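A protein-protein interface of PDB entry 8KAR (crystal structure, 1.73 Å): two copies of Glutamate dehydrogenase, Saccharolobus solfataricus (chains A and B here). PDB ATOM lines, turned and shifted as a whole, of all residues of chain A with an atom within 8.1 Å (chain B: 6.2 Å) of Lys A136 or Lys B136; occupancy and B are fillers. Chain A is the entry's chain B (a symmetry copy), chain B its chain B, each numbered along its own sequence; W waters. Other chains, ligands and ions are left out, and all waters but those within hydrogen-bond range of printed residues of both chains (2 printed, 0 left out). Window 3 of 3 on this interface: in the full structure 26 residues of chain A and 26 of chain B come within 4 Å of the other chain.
The side-chain hydroxyl (OH) of Tyr B137 sits at hydrogen-bond distance from the backbone NH (N) of His A135 (3.4 Å).
The side-chain hydroxyl (OH) of Tyr B137 is in hydrogen-bond range of the backbone NH (N) of Lys A136, 3.1 Å away.
The backbone NH (N) of His B135 lies within hydrogen-bond range of the side-chain hydroxyl (OH) of Tyr A137, 3.4 Å away.
O of Leu B133 is in hydrogen-bond range of NH2 of Arg A39 (2.8 Å).
OH of Tyr A137 lies within hydrogen-bond range of N of Lys B136, at 3.1 Å.
O of Leu B133 lies within hydrogen-bond range of OH of Tyr A137 (3.0 Å).
OH of Tyr B137 lies within hydrogen-bond range of O of Leu A133.
ND1 of His B135 lies within hydrogen-bond range of O of Gln B132, at 2.9 Å.
O of Gln A132 lies within hydrogen-bond range of ND1 of His A135 (2.9 Å).
The side-chain amide nitrogen (NE2) of Gln A63 lies within hydrogen-bond range of the backbone carbonyl oxygen (O) of Tyr A137, 2.9 Å away.
N of Gln A63 is in hydrogen-bond range of O of Arg A39, 2.7 Å away.
Ile A134 touches Tyr B137.
Lys A136 touches Lys B136.
Tyr A137 touches Ile B134.
CD2 of Tyr B137 touches CD2 of Tyr A137, at 3.6 Å.
Printed residues of chain B within 4 Å of Leu A133: Tyr B137.
Printed residues of chain B within 4 Å of Ile A134: Tyr B137.
Of chain B, only Lys B136 and Tyr B137 come within 4 Å of Lys A136.
Val B131 touches none of the printed residues of chain A.
Printed residues of chain A within 4 Å of Leu B133: Arg A39 (2.8 Å) and Tyr A137 (3.0 Å).
Printed residues of chain A within 4 Å of Ile B134: Tyr A137.
Lys B136 touches just these residues of chain A: Lys A136 and Tyr A137.
Of the printed residues of chain A, Tyr B137 touches Leu A133 (3.0 Å), Ile A134 (3.1 Å), His A135 (3.4 Å), Lys A136 (3.1 Å) and Tyr A137 (3.6 Å).
The nearest residue of chain A that does not touch Lys B136 is Arg A39 (6.5 Å).
The nearest printed residue of chain A that does not touch Leu B133 is Gln A63 (6.8 Å).
Of the 9 printed residues of chain B, 5 touch a printed residue of chain A.
Hydrophobic or aromatic side chains of chain B within 4 Å of the printed part of chain A: Tyr B137.
Of the 17 printed residues of chain A, 6 touch a printed residue of chain B.
Hydrophobic or aromatic side chains of chain A within 4 Å of the printed part of chain B: Tyr A137.
Among the printed residues, no Asp or Glu carboxylate lies within 4 Å of a Lys or Arg side-chain nitrogen of the other chain.
Ile A134 touches Tyr B137, and with the chains exchanged Tyr A137 touches Ile B134.
Lys A136 touches its own counterpart, Lys B136.
Lys A136 touches Tyr B137, and with the chains exchanged Tyr A137 touches Lys B136.
Tyr B137 touches its own counterpart, Tyr A137.
9 positions are printed for both chains.
Of the 11 pairs that touch across the chains among the printed residues, 10 have their exchanged pair printed and touching as well.
Water W2 lies within hydrogen-bond range of OH of Tyr B137 (2.6 Å), O of Gln A132 (2.6 Å) and O of Leu A133 (3.1 Å).
Water W1 lies within hydrogen-bond range of OH of Tyr A137 (2.6 Å), O of Gln B132 (2.6 Å), NH2 of Arg A39 (3.0 Å) and O of Leu B133 (3.1 Å).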
ATOM      1  N   ARG A  39      30.522 -14.602 -23.936  1.00  0.00           N
ATOM      2  CA  ARG A  39      29.087 -14.668 -23.960  1.00  0.00           C
ATOM      3  C   ARG A  39      28.419 -13.448 -23.283  1.00  0.00           C
ATOM      4  O   ARG A  39      28.863 -12.987 -22.263  1.00  0.00           O
ATOM      5  CB  ARG A  39      28.537 -15.924 -23.230  1.00  0.00           C
ATOM      6  CG  ARG A  39      27.039 -16.096 -23.267  1.00  0.00           C
ATOM      7  CD  ARG A  39      26.667 -17.343 -22.474  1.00  0.00           C
ATOM      8  NE  ARG A  39      27.326 -18.512 -23.037  1.00  0.00           N
ATOM      9  CZ  ARG A  39      28.392 -19.107 -22.522  1.00  0.00           C
ATOM     10  NH1 ARG A  39      28.950 -18.665 -21.409  1.00  0.00           N
ATOM     11  NH2 ARG A  39      28.902 -20.150 -23.137  1.00  0.00           N
ATOM     12  N   MET A  41      24.449 -12.128 -22.237  1.00  0.00           N
ATOM     13  CA  MET A  41      23.039 -12.378 -22.261  1.00  0.00           C
ATOM     14  C   MET A  41      22.310 -11.089 -21.971  1.00  0.00           C
ATOM     15  O   MET A  41      22.651 -10.395 -21.003  1.00  0.00           O
ATOM     16  CB  MET A  41      22.564 -13.378 -21.199  1.00  0.00           C
ATOM     17  CG  MET A  41      23.104 -14.731 -21.450  1.00  0.00           C
ATOM     18  SD  MET A  41      22.916 -15.935 -20.127  1.00  0.00           S
ATOM     19  CE  MET A  41      24.179 -15.353 -18.975  1.00  0.00           C
ATOM     20  N   GLN A  63      29.833 -12.141 -19.888  1.00  0.00           N
ATOM     21  CA  GLN A  63      30.746 -13.175 -19.430  1.00  0.00           C
ATOM     22  C   GLN A  63      31.892 -12.987 -20.388  1.00  0.00           C
ATOM     23  O   GLN A  63      31.846 -13.463 -21.490  1.00  0.00           O
ATOM     24  CB  GLN A  63      30.061 -14.486 -19.611  1.00  0.00           C
ATOM     25  CG  GLN A  63      28.786 -14.534 -18.768  1.00  0.00           C
ATOM     26  CD  GLN A  63      28.128 -15.896 -18.714  1.00  0.00           C
ATOM     27  OE1 GLN A  63      28.011 -16.577 -19.721  1.00  0.00           O
ATOM     28  NE2 GLN A  63      27.643 -16.274 -17.526  1.00  0.00           N
ATOM     29  N   VAL A 131      17.948 -13.349 -12.086  1.00  0.00           N
ATOM     30  CA  VAL A 131      18.625 -14.638 -11.880  1.00  0.00           C
ATOM     31  C   VAL A 131      17.915 -15.762 -12.625  1.00  0.00           C
ATOM     32  O   VAL A 131      18.581 -16.647 -13.190  1.00  0.00           O
ATOM     33  CB  VAL A 131      18.790 -14.972 -10.387  1.00  0.00           C
ATOM     34  CG1 VAL A 131      19.034 -16.467 -10.096  1.00  0.00           C
ATOM     35  CG2 VAL A 131      19.916 -14.109  -9.831  1.00  0.00           C
ATOM     36  N   GLN A 132      16.587 -15.783 -12.564  1.00  0.00           N
ATOM     37  CA  GLN A 132      15.870 -16.840 -13.262  1.00  0.00           C
ATOM     38  C   GLN A 132      16.220 -16.866 -14.754  1.00  0.00           C
ATOM     39  O   GLN A 132      16.407 -17.919 -15.332  1.00  0.00           O
ATOM     40  CB  GLN A 132      14.362 -16.789 -13.038  1.00  0.00           C
ATOM     41  CG  GLN A 132      13.670 -18.092 -13.426  1.00  0.00           C
ATOM     42  CD  GLN A 132      13.422 -18.217 -14.918  1.00  0.00           C
ATOM     43  OE1 GLN A 132      13.447 -17.221 -15.626  1.00  0.00           O
ATOM     44  NE2 GLN A 132      13.292 -19.445 -15.412  1.00  0.00           N
ATOM     45  N   LEU A 133      16.353 -15.714 -15.397  1.00  0.00           N
ATOM     46  CA  LEU A 133      16.402 -15.678 -16.851  1.00  0.00           C
ATOM     47  C   LEU A 133      17.798 -16.010 -17.399  1.00  0.00           C
ATOM     48  O   LEU A 133      17.888 -16.426 -18.554  1.00  0.00           O
ATOM     49  CB  LEU A 133      15.924 -14.289 -17.295  1.00  0.00           C
ATOM     50  CG  LEU A 133      14.414 -14.073 -17.203  1.00  0.00           C
ATOM     51  CD1 LEU A 133      14.049 -12.606 -17.175  1.00  0.00           C
ATOM     52  CD2 LEU A 133      13.702 -14.756 -18.369  1.00  0.00           C
ATOM     53  N   ILE A 134      18.836 -15.928 -16.552  1.00  0.00           N
ATOM     54  CA  ILE A 134      20.189 -16.277 -16.934  1.00  0.00           C
ATOM     55  C   ILE A 134      20.722 -17.549 -16.226  1.00  0.00           C
ATOM     56  O   ILE A 134      21.867 -17.921 -16.487  1.00  0.00           O
ATOM     57  CB  ILE A 134      21.112 -15.076 -16.675  1.00  0.00           C
ATOM     58  CG1 ILE A 134      21.307 -14.874 -15.167  1.00  0.00           C
ATOM     59  CG2 ILE A 134      20.588 -13.837 -17.393  1.00  0.00           C
ATOM     60  CD1 ILE A 134      22.383 -13.872 -14.813  1.00  0.00           C
ATOM     61  N   HIS A 135      19.981 -18.165 -15.299  1.00  0.00           N
ATOM     62  CA  HIS A 135      20.537 -19.168 -14.376  1.00  0.00           C
ATOM     63  C   HIS A 135      21.231 -20.345 -15.082  1.00  0.00           C
ATOM     64  O   HIS A 135      22.094 -20.987 -14.503  1.00  0.00           O
ATOM     65  CB  HIS A 135      19.532 -19.648 -13.289  1.00  0.00           C
ATOM     66  CG  HIS A 135      18.649 -20.732 -13.797  1.00  0.00           C
ATOM     67  ND1 HIS A 135      17.524 -20.467 -14.541  1.00  0.00           N
ATOM     68  CD2 HIS A 135      18.756 -22.085 -13.695  1.00  0.00           C
ATOM     69  CE1 HIS A 135      16.971 -21.633 -14.887  1.00  0.00           C
ATOM     70  NE2 HIS A 135      17.711 -22.639 -14.407  1.00  0.00           N
ATOM     71  N   LYS A 136      20.808 -20.759 -16.294  1.00  0.00           N
ATOM     72  CA  LYS A 136      21.453 -21.867 -16.931  1.00  0.00           C
ATOM     73  C   LYS A 136      22.924 -21.565 -17.265  1.00  0.00           C
ATOM     74  O   LYS A 136      23.676 -22.524 -17.537  1.00  0.00           O
ATOM     75  CB  LYS A 136      20.735 -22.282 -18.229  1.00  0.00           C
ATOM     76  CG  LYS A 136      19.326 -22.778 -18.067  1.00  0.00           C
ATOM     77  CD  LYS A 136      19.202 -24.071 -17.291  1.00  0.00           C
ATOM     78  CE  LYS A 136      17.796 -24.635 -17.351  1.00  0.00           C
ATOM     79  NZ  LYS A 136      17.691 -25.945 -16.659  1.00  0.00           N
ATOM     80  N   TYR A 137      23.355 -20.282 -17.212  1.00  0.00           N
ATOM     81  CA  TYR A 137      24.761 -19.898 -17.384  1.00  0.00           C
ATOM     82  C   TYR A 137      25.332 -19.244 -16.115  1.00  0.00           C
ATOM     83  O   TYR A 137      26.286 -18.453 -16.194  1.00  0.00           O
ATOM     84  CB  TYR A 137      25.024 -19.010 -18.601  1.00  0.00           C
ATOM     85  CG  TYR A 137      25.157 -19.748 -19.905  1.00  0.00           C
ATOM     86  CD1 TYR A 137      26.232 -20.616 -20.110  1.00  0.00           C
ATOM     87  CD2 TYR A 137      24.141 -19.742 -20.840  1.00  0.00           C
ATOM     88  CE1 TYR A 137      26.363 -21.355 -21.272  1.00  0.00           C
ATOM     89  CE2 TYR A 137      24.251 -20.471 -22.007  1.00  0.00           C
ATOM     90  CZ  TYR A 137      25.331 -21.324 -22.188  1.00  0.00           C
ATOM     91  OH  TYR A 137      25.420 -22.042 -23.325  1.00  0.00           O
ATOM     92  N   LEU A 138      24.687 -19.515 -14.976  1.00  0.00           N
ATOM     93  CA  LEU A 138      25.281 -19.256 -13.650  1.00  0.00           C
ATOM     94  C   LEU A 138      25.625 -20.580 -12.920  1.00  0.00           C
ATOM     95  O   LEU A 138      25.154 -21.631 -13.277  1.00  0.00           O
ATOM     96  CB  LEU A 138      24.265 -18.489 -12.802  1.00  0.00           C
ATOM     97  CG  LEU A 138      23.908 -17.074 -13.238  1.00  0.00           C
ATOM     98  CD1 LEU A 138      22.909 -16.493 -12.235  1.00  0.00           C
ATOM     99  CD2 LEU A 138      25.116 -16.176 -13.428  1.00  0.00           C
ATOM    100  N   GLY A 139      26.388 -20.512 -11.799  1.00  0.00           N
ATOM    101  CA  GLY A 139      26.780 -21.678 -11.028  1.00  0.00           C
ATOM    102  C   GLY A 139      28.075 -21.378 -10.280  1.00  0.00           C
ATOM    103  O   GLY A 139      28.862 -20.532 -10.720  1.00  0.00           O
ATOM    104  N   VAL A 142      30.738 -21.719 -12.625  1.00  0.00           N
ATOM    105  CA  VAL A 142      30.351 -21.243 -13.929  1.00  0.00           C
ATOM    106  C   VAL A 142      30.450 -19.725 -13.971  1.00  0.00           C
ATOM    107  O   VAL A 142      31.223 -19.169 -14.749  1.00  0.00           O
ATOM    108  CB  VAL A 142      28.938 -21.724 -14.310  1.00  0.00           C
ATOM    109  CG1 VAL A 142      28.457 -21.051 -15.589  1.00  0.00           C
ATOM    110  CG2 VAL A 142      28.837 -23.237 -14.373  1.00  0.00           C
ATOM    111  N   ASP A 143      29.645 -19.060 -13.141  1.00  0.00           N
ATOM    112  CA  ASP A 143      29.591 -17.596 -13.044  1.00  0.00           C
ATOM    113  C   ASP A 143      28.971 -17.214 -11.706  1.00  0.00           C
ATOM    114  O   ASP A 143      27.852 -17.590 -11.392  1.00  0.00           O
ATOM    115  CB  ASP A 143      28.780 -16.996 -14.177  1.00  0.00           C
ATOM    116  CG  ASP A 143      28.791 -15.480 -14.251  1.00  0.00           C
ATOM    117  OD1 ASP A 143      29.469 -14.776 -13.393  1.00  0.00           O
ATOM    118  OD2 ASP A 143      28.129 -15.018 -15.138  1.00  0.00           O
ATOM    119  N   TYR A 163      17.796 -18.883  -6.775  1.00  0.00           N
ATOM    120  CA  TYR A 163      18.667 -19.897  -7.336  1.00  0.00           C
ATOM    121  C   TYR A 163      18.397 -21.232  -6.645  1.00  0.00           C
ATOM    122  O   TYR A 163      18.303 -22.214  -7.329  1.00  0.00           O
ATOM    123  CB  TYR A 163      20.139 -19.534  -7.206  1.00  0.00           C
ATOM    124  CG  TYR A 163      21.037 -20.532  -7.883  1.00  0.00           C
ATOM    125  CD1 TYR A 163      21.424 -21.696  -7.223  1.00  0.00           C
ATOM    126  CD2 TYR A 163      21.426 -20.355  -9.205  1.00  0.00           C
ATOM    127  CE1 TYR A 163      22.196 -22.663  -7.855  1.00  0.00           C
ATOM    128  CE2 TYR A 163      22.225 -21.297  -9.839  1.00  0.00           C
ATOM    129  CZ  TYR A 163      22.630 -22.432  -9.149  1.00  0.00           C
ATOM    130  OH  TYR A 163      23.434 -23.347  -9.771  1.00  0.00           O
ATOM    131  N   ILE A 166      15.050 -22.621  -7.943  1.00  0.00           N
ATOM    132  CA  ILE A 166      15.079 -23.156  -9.300  1.00  0.00           C
ATOM    133  C   ILE A 166      15.870 -24.479  -9.332  1.00  0.00           C
ATOM    134  O   ILE A 166      15.489 -25.376 -10.065  1.00  0.00           O
ATOM    135  CB  ILE A 166      15.717 -22.108 -10.242  1.00  0.00           C
ATOM    136  CG1 ILE A 166      14.831 -20.870 -10.438  1.00  0.00           C
ATOM    137  CG2 ILE A 166      16.177 -22.728 -11.553  1.00  0.00           C
ATOM    138  CD1 ILE A 166      15.668 -19.702 -10.964  1.00  0.00           C
ATOM    139  N   THR A 167      16.973 -24.576  -8.588  1.00  0.00           N
ATOM    140  CA  THR A 167      17.931 -25.669  -8.788  1.00  0.00           C
ATOM    141  C   THR A 167      17.688 -26.736  -7.717  1.00  0.00           C
ATOM    142  O   THR A 167      18.032 -27.904  -7.895  1.00  0.00           O
ATOM    143  CB  THR A 167      19.393 -25.211  -8.788  1.00  0.00           C
ATOM    144  OG1 THR A 167      19.734 -24.843  -7.432  1.00  0.00           O
ATOM    145  CG2 THR A 167      19.706 -24.111  -9.791  1.00  0.00           C
ATOM    146  N   VAL B 131      27.005 -23.568 -31.725  1.00  0.00           N
ATOM    147  CA  VAL B 131      26.150 -24.429 -30.894  1.00  0.00           C
ATOM    148  C   VAL B 131      26.752 -24.633 -29.508  1.00  0.00           C
ATOM    149  O   VAL B 131      26.011 -24.648 -28.509  1.00  0.00           O
ATOM    150  CB  VAL B 131      25.847 -25.774 -31.577  1.00  0.00           C
ATOM    151  CG1 VAL B 131      25.389 -26.885 -30.610  1.00  0.00           C
ATOM    152  CG2 VAL B 131      24.813 -25.528 -32.667  1.00  0.00           C
ATOM    153  N   GLN B 132      28.059 -24.870 -29.445  1.00  0.00           N
ATOM    154  CA  GLN B 132      28.672 -25.070 -28.141  1.00  0.00           C
ATOM    155  C   GLN B 132      28.417 -23.878 -27.211  1.00  0.00           C
ATOM    156  O   GLN B 132      28.130 -24.050 -26.042  1.00  0.00           O
ATOM    157  CB  GLN B 132      30.156 -25.413 -28.223  1.00  0.00           C
ATOM    158  CG  GLN B 132      30.693 -26.002 -26.922  1.00  0.00           C
ATOM    159  CD  GLN B 132      31.016 -24.950 -25.878  1.00  0.00           C
ATOM    160  OE1 GLN B 132      31.170 -23.785 -26.212  1.00  0.00           O
ATOM    161  NE2 GLN B 132      31.013 -25.337 -24.604  1.00  0.00           N
ATOM    162  N   LEU B 133      28.480 -22.653 -27.714  1.00  0.00           N
ATOM    163  CA  LEU B 133      28.529 -21.493 -26.838  1.00  0.00           C
ATOM    164  C   LEU B 133      27.140 -21.085 -26.326  1.00  0.00           C
ATOM    165  O   LEU B 133      27.069 -20.429 -25.287  1.00  0.00           O
ATOM    166  CB  LEU B 133      29.215 -20.358 -27.611  1.00  0.00           C
ATOM    167  CG  LEU B 133      30.731 -20.498 -27.740  1.00  0.00           C
ATOM    168  CD1 LEU B 133      31.285 -19.668 -28.876  1.00  0.00           C
ATOM    169  CD2 LEU B 133      31.419 -20.104 -26.434  1.00  0.00           C
ATOM    170  N   ILE B 134      26.070 -21.556 -26.986  1.00  0.00           N
ATOM    171  CA  ILE B 134      24.710 -21.293 -26.562  1.00  0.00           C
ATOM    172  C   ILE B 134      23.969 -22.554 -26.048  1.00  0.00           C
ATOM    173  O   ILE B 134      22.803 -22.427 -25.668  1.00  0.00           O
ATOM    174  CB  ILE B 134      23.939 -20.636 -27.717  1.00  0.00           C
ATOM    175  CG1 ILE B 134      23.677 -21.659 -28.829  1.00  0.00           C
ATOM    176  CG2 ILE B 134      24.668 -19.385 -28.200  1.00  0.00           C
ATOM    177  CD1 ILE B 134      22.724 -21.177 -29.899  1.00  0.00           C
ATOM    178  N   HIS B 135      24.560 -23.752 -26.100  1.00  0.00           N
ATOM    179  CA  HIS B 135      23.818 -25.012 -25.931  1.00  0.00           C
ATOM    180  C   HIS B 135      23.020 -25.093 -24.618  1.00  0.00           C
ATOM    181  O   HIS B 135      22.045 -25.823 -24.535  1.00  0.00           O
ATOM    182  CB  HIS B 135      24.679 -26.286 -26.172  1.00  0.00           C
ATOM    183  CG  HIS B 135      25.441 -26.673 -24.954  1.00  0.00           C
ATOM    184  ND1 HIS B 135      26.636 -26.081 -24.624  1.00  0.00           N
ATOM    185  CD2 HIS B 135      25.149 -27.569 -23.972  1.00  0.00           C
ATOM    186  CE1 HIS B 135      27.051 -26.600 -23.465  1.00  0.00           C
ATOM    187  NE2 HIS B 135      26.155 -27.493 -23.029  1.00  0.00           N
ATOM    188  N   LYS B 136      23.462 -24.460 -23.512  1.00  0.00           N
ATOM    189  CA  LYS B 136      22.717 -24.557 -22.294  1.00  0.00           C
ATOM    190  C   LYS B 136      21.324 -23.917 -22.414  1.00  0.00           C
ATOM    191  O   LYS B 136      20.471 -24.195 -21.546  1.00  0.00           O
ATOM    192  CB  LYS B 136      23.456 -23.897 -21.113  1.00  0.00           C
ATOM    193  CG  LYS B 136      24.774 -24.515 -20.738  1.00  0.00           C
ATOM    194  CD  LYS B 136      24.675 -25.928 -20.209  1.00  0.00           C
ATOM    195  CE  LYS B 136      25.994 -26.415 -19.642  1.00  0.00           C
ATOM    196  NZ  LYS B 136      25.880 -27.771 -19.048  1.00  0.00           N
ATOM    197  N   TYR B 137      21.065 -23.114 -23.474  1.00  0.00           N
ATOM    198  CA  TYR B 137      19.736 -22.558 -23.755  1.00  0.00           C
ATOM    199  C   TYR B 137      19.177 -23.068 -25.093  1.00  0.00           C
ATOM    200  O   TYR B 137      18.344 -22.395 -25.721  1.00  0.00           O
ATOM    201  CB  TYR B 137      19.672 -21.031 -23.703  1.00  0.00           C
ATOM    202  CG  TYR B 137      19.525 -20.451 -22.323  1.00  0.00           C
ATOM    203  CD1 TYR B 137      18.361 -20.682 -21.588  1.00  0.00           C
ATOM    204  CD2 TYR B 137      20.591 -19.854 -21.678  1.00  0.00           C
ATOM    205  CE1 TYR B 137      18.207 -20.213 -20.295  1.00  0.00           C
ATOM    206  CE2 TYR B 137      20.460 -19.379 -20.389  1.00  0.00           C
ATOM    207  CZ  TYR B 137      19.291 -19.618 -19.681  1.00  0.00           C
ATOM    208  OH  TYR B 137      19.180 -19.162 -18.418  1.00  0.00           O
ATOM    209  N   LEU B 138      19.706 -24.207 -25.552  1.00  0.00           N
ATOM    210  CA  LEU B 138      19.068 -25.001 -26.619  1.00  0.00           C
ATOM    211  C   LEU B 138      18.505 -26.337 -26.068  1.00  0.00           C
ATOM    212  O   LEU B 138      18.854 -26.766 -24.996  1.00  0.00           O
ATOM    213  CB  LEU B 138      20.121 -25.326 -27.681  1.00  0.00           C
ATOM    214  CG  LEU B 138      20.689 -24.165 -28.487  1.00  0.00           C
ATOM    215  CD1 LEU B 138      21.690 -24.723 -29.502  1.00  0.00           C
ATOM    216  CD2 LEU B 138      19.625 -23.306 -29.145  1.00  0.00           C
ATOM    217  N   VAL B 142      13.278 -26.586 -25.692  1.00  0.00           N
ATOM    218  CA  VAL B 142      13.807 -25.330 -25.223  1.00  0.00           C
ATOM    219  C   VAL B 142      13.914 -24.354 -26.385  1.00  0.00           C
ATOM    220  O   VAL B 142      13.272 -23.304 -26.381  1.00  0.00           O
ATOM    221  CB  VAL B 142      15.165 -25.517 -24.521  1.00  0.00           C
ATOM    222  CG1 VAL B 142      15.812 -24.173 -24.215  1.00  0.00           C
ATOM    223  CG2 VAL B 142      15.069 -26.410 -23.297  1.00  0.00           C
HETATM  224  O   HOH W   1      27.873 -22.913 -23.666  1.00  0.00           O
HETATM  225  O   HOH W   2      16.660 -19.106 -17.684  1.00  0.00           O
